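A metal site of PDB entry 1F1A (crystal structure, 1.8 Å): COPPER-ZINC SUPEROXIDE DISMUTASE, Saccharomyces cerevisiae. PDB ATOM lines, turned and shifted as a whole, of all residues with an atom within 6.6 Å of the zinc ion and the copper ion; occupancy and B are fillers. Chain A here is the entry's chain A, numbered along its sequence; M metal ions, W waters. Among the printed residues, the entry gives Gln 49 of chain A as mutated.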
ATOM      1  N   GLY A  45      34.878   3.334   0.551  1.00  0.00           N
ATOM      2  CA  GLY A  45      33.820   2.402   0.177  1.00  0.00           C
ATOM      3  C   GLY A  45      32.445   3.076   0.199  1.00  0.00           C
ATOM      4  O   GLY A  45      32.072   3.680   1.189  1.00  0.00           O
ATOM      5  N   PHE A  46      31.664   2.879  -0.859  1.00  0.00           N
ATOM      6  CA  PHE A  46      30.351   3.482  -1.029  1.00  0.00           C
ATOM      7  C   PHE A  46      29.395   2.331  -1.397  1.00  0.00           C
ATOM      8  O   PHE A  46      29.464   1.801  -2.496  1.00  0.00           O
ATOM      9  CB  PHE A  46      30.499   4.481  -2.197  1.00  0.00           C
ATOM     10  CG  PHE A  46      29.325   5.375  -2.422  1.00  0.00           C
ATOM     11  CD1 PHE A  46      28.652   5.966  -1.358  1.00  0.00           C
ATOM     12  CD2 PHE A  46      28.928   5.685  -3.718  1.00  0.00           C
ATOM     13  CE1 PHE A  46      27.603   6.867  -1.594  1.00  0.00           C
ATOM     14  CE2 PHE A  46      27.899   6.591  -3.967  1.00  0.00           C
ATOM     15  CZ  PHE A  46      27.235   7.178  -2.906  1.00  0.00           C
ATOM     16  N   HIS A  47      28.531   1.917  -0.466  1.00  0.00           N
ATOM     17  CA  HIS A  47      27.663   0.769  -0.719  1.00  0.00           C
ATOM     18  C   HIS A  47      26.224   0.936  -0.271  1.00  0.00           C
ATOM     19  O   HIS A  47      25.918   1.786   0.550  1.00  0.00           O
ATOM     20  CB  HIS A  47      28.204  -0.470   0.007  1.00  0.00           C
ATOM     21  CG  HIS A  47      29.679  -0.696  -0.178  1.00  0.00           C
ATOM     22  ND1 HIS A  47      30.549  -0.907   0.880  1.00  0.00           N
ATOM     23  CD2 HIS A  47      30.444  -0.678  -1.297  1.00  0.00           C
ATOM     24  CE1 HIS A  47      31.775  -0.990   0.407  1.00  0.00           C
ATOM     25  NE2 HIS A  47      31.742  -0.857  -0.907  1.00  0.00           N
ATOM     26  N   ILE A  48      25.358   0.092  -0.821  1.00  0.00           N
ATOM     27  CA  ILE A  48      23.946   0.048  -0.459  1.00  0.00           C
ATOM     28  C   ILE A  48      23.777  -1.209   0.385  1.00  0.00           C
ATOM     29  O   ILE A  48      24.226  -2.292  -0.009  1.00  0.00           O
ATOM     30  CB  ILE A  48      23.004  -0.002  -1.691  1.00  0.00           C
ATOM     31  CG1 ILE A  48      23.179   1.260  -2.523  1.00  0.00           C
ATOM     32  CG2 ILE A  48      21.546  -0.136  -1.256  1.00  0.00           C
ATOM     33  CD1 ILE A  48      22.266   1.329  -3.694  1.00  0.00           C
ATOM     34  N   GLN A  49      23.211  -1.039   1.582  1.00  0.00           N
ATOM     35  CA  GLN A  49      22.975  -2.119   2.539  1.00  0.00           C
ATOM     36  C   GLN A  49      21.590  -2.751   2.333  1.00  0.00           C
ATOM     37  O   GLN A  49      20.716  -2.132   1.737  1.00  0.00           O
ATOM     38  CB  GLN A  49      23.092  -1.579   3.954  1.00  0.00           C
ATOM     39  CG  GLN A  49      24.312  -0.734   4.210  1.00  0.00           C
ATOM     40  CD  GLN A  49      25.614  -1.524   4.157  1.00  0.00           C
ATOM     41  OE1 GLN A  49      26.658  -0.992   3.748  1.00  0.00           O
ATOM     42  NE2 GLN A  49      25.575  -2.782   4.594  1.00  0.00           N
ATOM     43  N   HIS A  64      25.642  -5.863   2.667  1.00  0.00           N
ATOM     44  CA  HIS A  64      25.397  -5.292   1.356  1.00  0.00           C
ATOM     45  C   HIS A  64      24.170  -5.944   0.719  1.00  0.00           C
ATOM     46  O   HIS A  64      23.948  -7.153   0.874  1.00  0.00           O
ATOM     47  CB  HIS A  64      26.599  -5.532   0.456  1.00  0.00           C
ATOM     48  CG  HIS A  64      27.803  -4.751   0.842  1.00  0.00           C
ATOM     49  ND1 HIS A  64      29.051  -4.982   0.318  1.00  0.00           N
ATOM     50  CD2 HIS A  64      27.947  -3.721   1.711  1.00  0.00           C
ATOM     51  CE1 HIS A  64      29.916  -4.140   0.835  1.00  0.00           C
ATOM     52  NE2 HIS A  64      29.274  -3.354   1.686  1.00  0.00           N
ATOM     53  N   PHE A  65      23.364  -5.133   0.021  1.00  0.00           N
ATOM     54  CA  PHE A  65      22.165  -5.638  -0.651  1.00  0.00           C
ATOM     55  C   PHE A  65      22.727  -6.643  -1.690  1.00  0.00           C
ATOM     56  O   PHE A  65      23.500  -6.286  -2.582  1.00  0.00           O
ATOM     57  CB  PHE A  65      21.390  -4.471  -1.305  1.00  0.00           C
ATOM     58  CG  PHE A  65      20.074  -4.878  -1.939  1.00  0.00           C
ATOM     59  CD1 PHE A  65      19.259  -5.847  -1.361  1.00  0.00           C
ATOM     60  CD2 PHE A  65      19.674  -4.302  -3.143  1.00  0.00           C
ATOM     61  CE1 PHE A  65      18.076  -6.246  -1.985  1.00  0.00           C
ATOM     62  CE2 PHE A  65      18.486  -4.706  -3.778  1.00  0.00           C
ATOM     63  CZ  PHE A  65      17.687  -5.678  -3.183  1.00  0.00           C
ATOM     64  N   THR A  71      29.438 -12.783  -4.521  1.00  0.00           N
ATOM     65  CA  THR A  71      30.482 -12.278  -3.644  1.00  0.00           C
ATOM     66  C   THR A  71      30.712 -10.801  -3.936  1.00  0.00           C
ATOM     67  O   THR A  71      30.291 -10.287  -4.964  1.00  0.00           O
ATOM     68  CB  THR A  71      31.811 -13.015  -3.812  1.00  0.00           C
ATOM     69  OG1 THR A  71      32.181 -13.005  -5.196  1.00  0.00           O
ATOM     70  CG2 THR A  71      31.702 -14.447  -3.330  1.00  0.00           C
ATOM     71  N   HIS A  72      31.380 -10.125  -2.999  1.00  0.00           N
ATOM     72  CA  HIS A  72      31.675  -8.697  -3.116  1.00  0.00           C
ATOM     73  C   HIS A  72      32.637  -8.420  -4.282  1.00  0.00           C
ATOM     74  O   HIS A  72      33.595  -9.152  -4.475  1.00  0.00           O
ATOM     75  CB  HIS A  72      32.299  -8.198  -1.802  1.00  0.00           C
ATOM     76  CG  HIS A  72      32.643  -6.745  -1.810  1.00  0.00           C
ATOM     77  ND1 HIS A  72      31.698  -5.760  -1.631  1.00  0.00           N
ATOM     78  CD2 HIS A  72      33.804  -6.121  -2.064  1.00  0.00           C
ATOM     79  CE1 HIS A  72      32.277  -4.579  -1.777  1.00  0.00           C
ATOM     80  NE2 HIS A  72      33.563  -4.775  -2.045  1.00  0.00           N
ATOM     81  N   GLY A  73      32.389  -7.346  -5.018  1.00  0.00           N
ATOM     82  CA  GLY A  73      33.261  -7.023  -6.139  1.00  0.00           C
ATOM     83  C   GLY A  73      33.206  -5.557  -6.478  1.00  0.00           C
ATOM     84  O   GLY A  73      32.660  -4.757  -5.729  1.00  0.00           O
ATOM     85  N   ARG A  80      29.388  -9.301  -8.363  1.00  0.00           N
ATOM     86  CA  ARG A  80      29.367  -8.233  -7.360  1.00  0.00           C
ATOM     87  C   ARG A  80      27.997  -8.267  -6.698  1.00  0.00           C
ATOM     88  O   ARG A  80      27.072  -8.939  -7.171  1.00  0.00           O
ATOM     89  CB  ARG A  80      29.524  -6.856  -8.025  1.00  0.00           C
ATOM     90  CG  ARG A  80      28.526  -6.630  -9.141  1.00  0.00           C
ATOM     91  CD  ARG A  80      28.489  -5.196  -9.648  1.00  0.00           C
ATOM     92  NE  ARG A  80      27.518  -4.373  -8.928  1.00  0.00           N
ATOM     93  CZ  ARG A  80      26.984  -3.240  -9.380  1.00  0.00           C
ATOM     94  NH1 ARG A  80      27.350  -2.778 -10.579  1.00  0.00           N
ATOM     95  NH2 ARG A  80      26.024  -2.619  -8.708  1.00  0.00           N
ATOM     96  N   HIS A  81      27.892  -7.590  -5.557  1.00  0.00           N
ATOM     97  CA  HIS A  81      26.609  -7.467  -4.872  1.00  0.00           C
ATOM     98  C   HIS A  81      25.907  -6.329  -5.606  1.00  0.00           C
ATOM     99  O   HIS A  81      26.569  -5.476  -6.188  1.00  0.00           O
ATOM    100  CB  HIS A  81      26.815  -7.043  -3.421  1.00  0.00           C
ATOM    101  CG  HIS A  81      27.505  -8.075  -2.589  1.00  0.00           C
ATOM    102  ND1 HIS A  81      28.316  -7.754  -1.533  1.00  0.00           N
ATOM    103  CD2 HIS A  81      27.450  -9.420  -2.639  1.00  0.00           C
ATOM    104  CE1 HIS A  81      28.735  -8.864  -0.952  1.00  0.00           C
ATOM    105  NE2 HIS A  81      28.224  -9.888  -1.607  1.00  0.00           N
ATOM    106  N   VAL A  82      24.583  -6.311  -5.585  1.00  0.00           N
ATOM    107  CA  VAL A  82      23.840  -5.232  -6.236  1.00  0.00           C
ATOM    108  C   VAL A  82      24.243  -3.872  -5.616  1.00  0.00           C
ATOM    109  O   VAL A  82      24.358  -2.881  -6.323  1.00  0.00           O
ATOM    110  CB  VAL A  82      22.324  -5.432  -6.077  1.00  0.00           C
ATOM    111  CG1 VAL A  82      21.572  -4.196  -6.524  1.00  0.00           C
ATOM    112  CG2 VAL A  82      21.894  -6.659  -6.869  1.00  0.00           C
ATOM    113  N   GLY A  83      24.473  -3.863  -4.307  1.00  0.00           N
ATOM    114  CA  GLY A  83      24.831  -2.640  -3.611  1.00  0.00           C
ATOM    115  C   GLY A  83      26.288  -2.223  -3.686  1.00  0.00           C
ATOM    116  O   GLY A  83      26.698  -1.289  -3.014  1.00  0.00           O
ATOM    117  N   ASP A  84      27.055  -2.916  -4.524  1.00  0.00           N
ATOM    118  CA  ASP A  84      28.473  -2.606  -4.643  1.00  0.00           C
ATOM    119  C   ASP A  84      28.747  -1.445  -5.588  1.00  0.00           C
ATOM    120  O   ASP A  84      28.839  -1.619  -6.794  1.00  0.00           O
ATOM    121  CB  ASP A  84      29.266  -3.850  -5.067  1.00  0.00           C
ATOM    122  CG  ASP A  84      29.502  -4.830  -3.900  1.00  0.00           C
ATOM    123  OD1 ASP A  84      29.204  -4.506  -2.717  1.00  0.00           O
ATOM    124  OD2 ASP A  84      30.003  -5.947  -4.143  1.00  0.00           O
ATOM    125  N   VAL A 119      25.577   3.599   2.652  1.00  0.00           N
ATOM    126  CA  VAL A 119      26.631   3.779   3.629  1.00  0.00           C
ATOM    127  C   VAL A 119      27.920   4.263   2.970  1.00  0.00           C
ATOM    128  O   VAL A 119      28.283   3.796   1.883  1.00  0.00           O
ATOM    129  CB  VAL A 119      26.937   2.425   4.378  1.00  0.00           C
ATOM    130  CG1 VAL A 119      28.300   2.476   5.029  1.00  0.00           C
ATOM    131  CG2 VAL A 119      25.887   2.167   5.437  1.00  0.00           C
ATOM    132  N   HIS A 121      31.824   4.478   3.775  1.00  0.00           N
ATOM    133  CA  HIS A 121      32.774   3.858   4.682  1.00  0.00           C
ATOM    134  C   HIS A 121      33.907   4.741   5.131  1.00  0.00           C
ATOM    135  O   HIS A 121      34.106   5.815   4.592  1.00  0.00           O
ATOM    136  CB  HIS A 121      33.330   2.580   4.084  1.00  0.00           C
ATOM    137  CG  HIS A 121      32.388   1.437   4.194  1.00  0.00           C
ATOM    138  ND1 HIS A 121      32.166   0.787   5.380  1.00  0.00           N
ATOM    139  CD2 HIS A 121      31.575   0.853   3.287  1.00  0.00           C
ATOM    140  CE1 HIS A 121      31.251  -0.160   5.202  1.00  0.00           C
ATOM    141  NE2 HIS A 121      30.883  -0.134   3.944  1.00  0.00           N
ATOM    142  N   ASP A 125      37.578   0.407  -0.210  1.00  0.00           N
ATOM    143  CA  ASP A 125      37.058  -0.887  -0.598  1.00  0.00           C
ATOM    144  C   ASP A 125      38.153  -1.569  -1.429  1.00  0.00           C
ATOM    145  O   ASP A 125      38.685  -0.950  -2.381  1.00  0.00           O
ATOM    146  CB  ASP A 125      35.791  -0.631  -1.443  1.00  0.00           C
ATOM    147  CG  ASP A 125      35.024  -1.906  -1.808  1.00  0.00           C
ATOM    148  OD1 ASP A 125      35.534  -3.035  -1.655  1.00  0.00           O
ATOM    149  OD2 ASP A 125      33.874  -1.750  -2.268  1.00  0.00           O
ATOM    150  N   LEU A 136      35.627 -10.775   0.259  1.00  0.00           N
ATOM    151  CA  LEU A 136      34.475 -11.238  -0.526  1.00  0.00           C
ATOM    152  C   LEU A 136      33.117 -10.918   0.097  1.00  0.00           C
ATOM    153  O   LEU A 136      32.079 -11.192  -0.496  1.00  0.00           O
ATOM    154  CB  LEU A 136      34.546 -12.748  -0.761  1.00  0.00           C
ATOM    155  CG  LEU A 136      35.746 -13.278  -1.543  1.00  0.00           C
ATOM    156  CD1 LEU A 136      35.606 -14.789  -1.630  1.00  0.00           C
ATOM    157  CD2 LEU A 136      35.809 -12.630  -2.917  1.00  0.00           C
ATOM    158  N   LYS A 137      33.135 -10.386   1.310  1.00  0.00           N
ATOM    159  CA  LYS A 137      31.925 -10.024   2.007  1.00  0.00           C
ATOM    160  C   LYS A 137      31.732  -8.519   2.036  1.00  0.00           C
ATOM    161  O   LYS A 137      30.766  -7.993   1.487  1.00  0.00           O
ATOM    162  CB  LYS A 137      31.961 -10.586   3.428  1.00  0.00           C
ATOM    163  CG  LYS A 137      31.525 -12.064   3.530  1.00  0.00           C
ATOM    164  CD  LYS A 137      30.110 -12.281   2.902  1.00  0.00           C
ATOM    165  CE  LYS A 137      30.147 -12.759   1.394  1.00  0.00           C
ATOM    166  NZ  LYS A 137      29.247 -11.980   0.407  1.00  0.00           N
ATOM    167  N   THR A 138      32.735  -7.809   2.552  1.00  0.00           N
ATOM    168  CA  THR A 138      32.646  -6.366   2.689  1.00  0.00           C
ATOM    169  C   THR A 138      33.688  -5.553   1.909  1.00  0.00           C
ATOM    170  O   THR A 138      33.583  -4.322   1.837  1.00  0.00           O
ATOM    171  CB  THR A 138      32.795  -5.968   4.174  1.00  0.00           C
ATOM    172  OG1 THR A 138      34.156  -6.211   4.593  1.00  0.00           O
ATOM    173  CG2 THR A 138      31.856  -6.782   5.053  1.00  0.00           C
ATOM    174  N   GLY A 139      34.666  -6.230   1.321  1.00  0.00           N
ATOM    175  CA  GLY A 139      35.696  -5.495   0.633  1.00  0.00           C
ATOM    176  C   GLY A 139      36.605  -4.846   1.666  1.00  0.00           C
ATOM    177  O   GLY A 139      37.441  -4.024   1.322  1.00  0.00           O
ATOM    178  N   ALA A 141      36.114  -2.592   3.847  1.00  0.00           N
ATOM    179  CA  ALA A 141      35.997  -1.128   3.877  1.00  0.00           C
ATOM    180  C   ALA A 141      35.930  -0.441   5.243  1.00  0.00           C
ATOM    181  O   ALA A 141      35.825   0.790   5.334  1.00  0.00           O
ATOM    182  CB  ALA A 141      34.857  -0.690   2.980  1.00  0.00           C
ATOM    183  N   GLY A 142      35.911  -1.212   6.310  1.00  0.00           N
ATOM    184  CA  GLY A 142      35.900  -0.623   7.627  1.00  0.00           C
ATOM    185  C   GLY A 142      34.568  -0.123   8.140  1.00  0.00           C
ATOM    186  O   GLY A 142      33.502  -0.513   7.639  1.00  0.00           O
ATOM    187  N   ARG A 144      31.337   2.469   9.386  1.00  0.00           N
ATOM    188  CA  ARG A 144      30.305   3.217   8.674  1.00  0.00           C
ATOM    189  C   ARG A 144      30.039   4.543   9.388  1.00  0.00           C
ATOM    190  O   ARG A 144      29.111   4.640  10.201  1.00  0.00           O
ATOM    191  CB  ARG A 144      29.016   2.408   8.664  1.00  0.00           C
ATOM    192  CG  ARG A 144      29.176   0.979   8.225  1.00  0.00           C
ATOM    193  CD  ARG A 144      27.890   0.213   8.427  1.00  0.00           C
ATOM    194  NE  ARG A 144      28.105  -1.186   8.109  1.00  0.00           N
ATOM    195  CZ  ARG A 144      27.149  -2.083   7.915  1.00  0.00           C
ATOM    196  NH1 ARG A 144      25.861  -1.746   7.975  1.00  0.00           N
ATOM    197  NH2 ARG A 144      27.494  -3.322   7.611  1.00  0.00           N
HETATM  198 ZN    ZN M   1      29.507  -5.809  -1.361  1.00  0.00          ZN
HETATM  199 CU    CU M   2      29.967  -1.690   2.791  1.00  0.00          CU
HETATM  200  O   HOH W   1      29.022  -2.223   4.378  1.00  0.00           O
HETATM  201  O   HOH W   2      31.949  -2.730   3.340  1.00  0.00           O
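O of His 47 is in hydrogen-bond range of N of Val 119 (2.8 Å). The backbone NH of His 121 sits at hydrogen-bond distance from the backbone carbonyl oxygen of Gly 45 (2.7 Å). The backbone NH of Gly 73 sits at hydrogen-bond distance from the side-chain carboxylate of Asp 84 (2.9 Å). NE2 of His 81 is in hydrogen-bond range of NZ of Lys 137. ND1 of His 121 sits at hydrogen-bond distance from O of Gly 142 (2.9 Å). NE2 of His 72 lies within hydrogen-bond range of OD1 of Asp 125, 2.7 Å away. OD2 of Asp 125 lies within hydrogen-bond range of NE2 of His 47 (2.7 Å). The backbone NH of His 72 sits at hydrogen-bond distance from the backbone carbonyl oxygen of Leu 136, at 2.8 Å.
O of Lys 137 touches the zinc ion (3.8 Å). Of the 25 residues printed, 5 come within 4 Å of the zinc ion.
Merely in contact with the copper ion: Gln 49 (3.5 Å). Four residues have an atom within 4 Å of the copper ion: His 47, Gln 49, His 64 and His 121.
OD1 of Asp 84 is bound to the zinc ion (1.9 Å). ND1 of His 64 is bound to the zinc ion, at 1.9 Å. The zinc ion is bound by ND1 of His 72 (2.2 Å). ND1 of His 81 binds the zinc ion (2.3 Å). Slightly farther from the zinc ion lies the side-chain carboxylate (OD2) of Asp 84 (2.8 Å).
The copper ion is bound by water W1 (1.9 Å). NE2 of His 64 binds the copper ion. The copper ion is bound by NE2 of His 121, at 2.1 Å. ND1 of His 47 is bound to the copper ion, at 2.1 Å. Water W2 is bound to the copper ion (2.3 Å). The copper ion has five donor atoms within binding distance.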
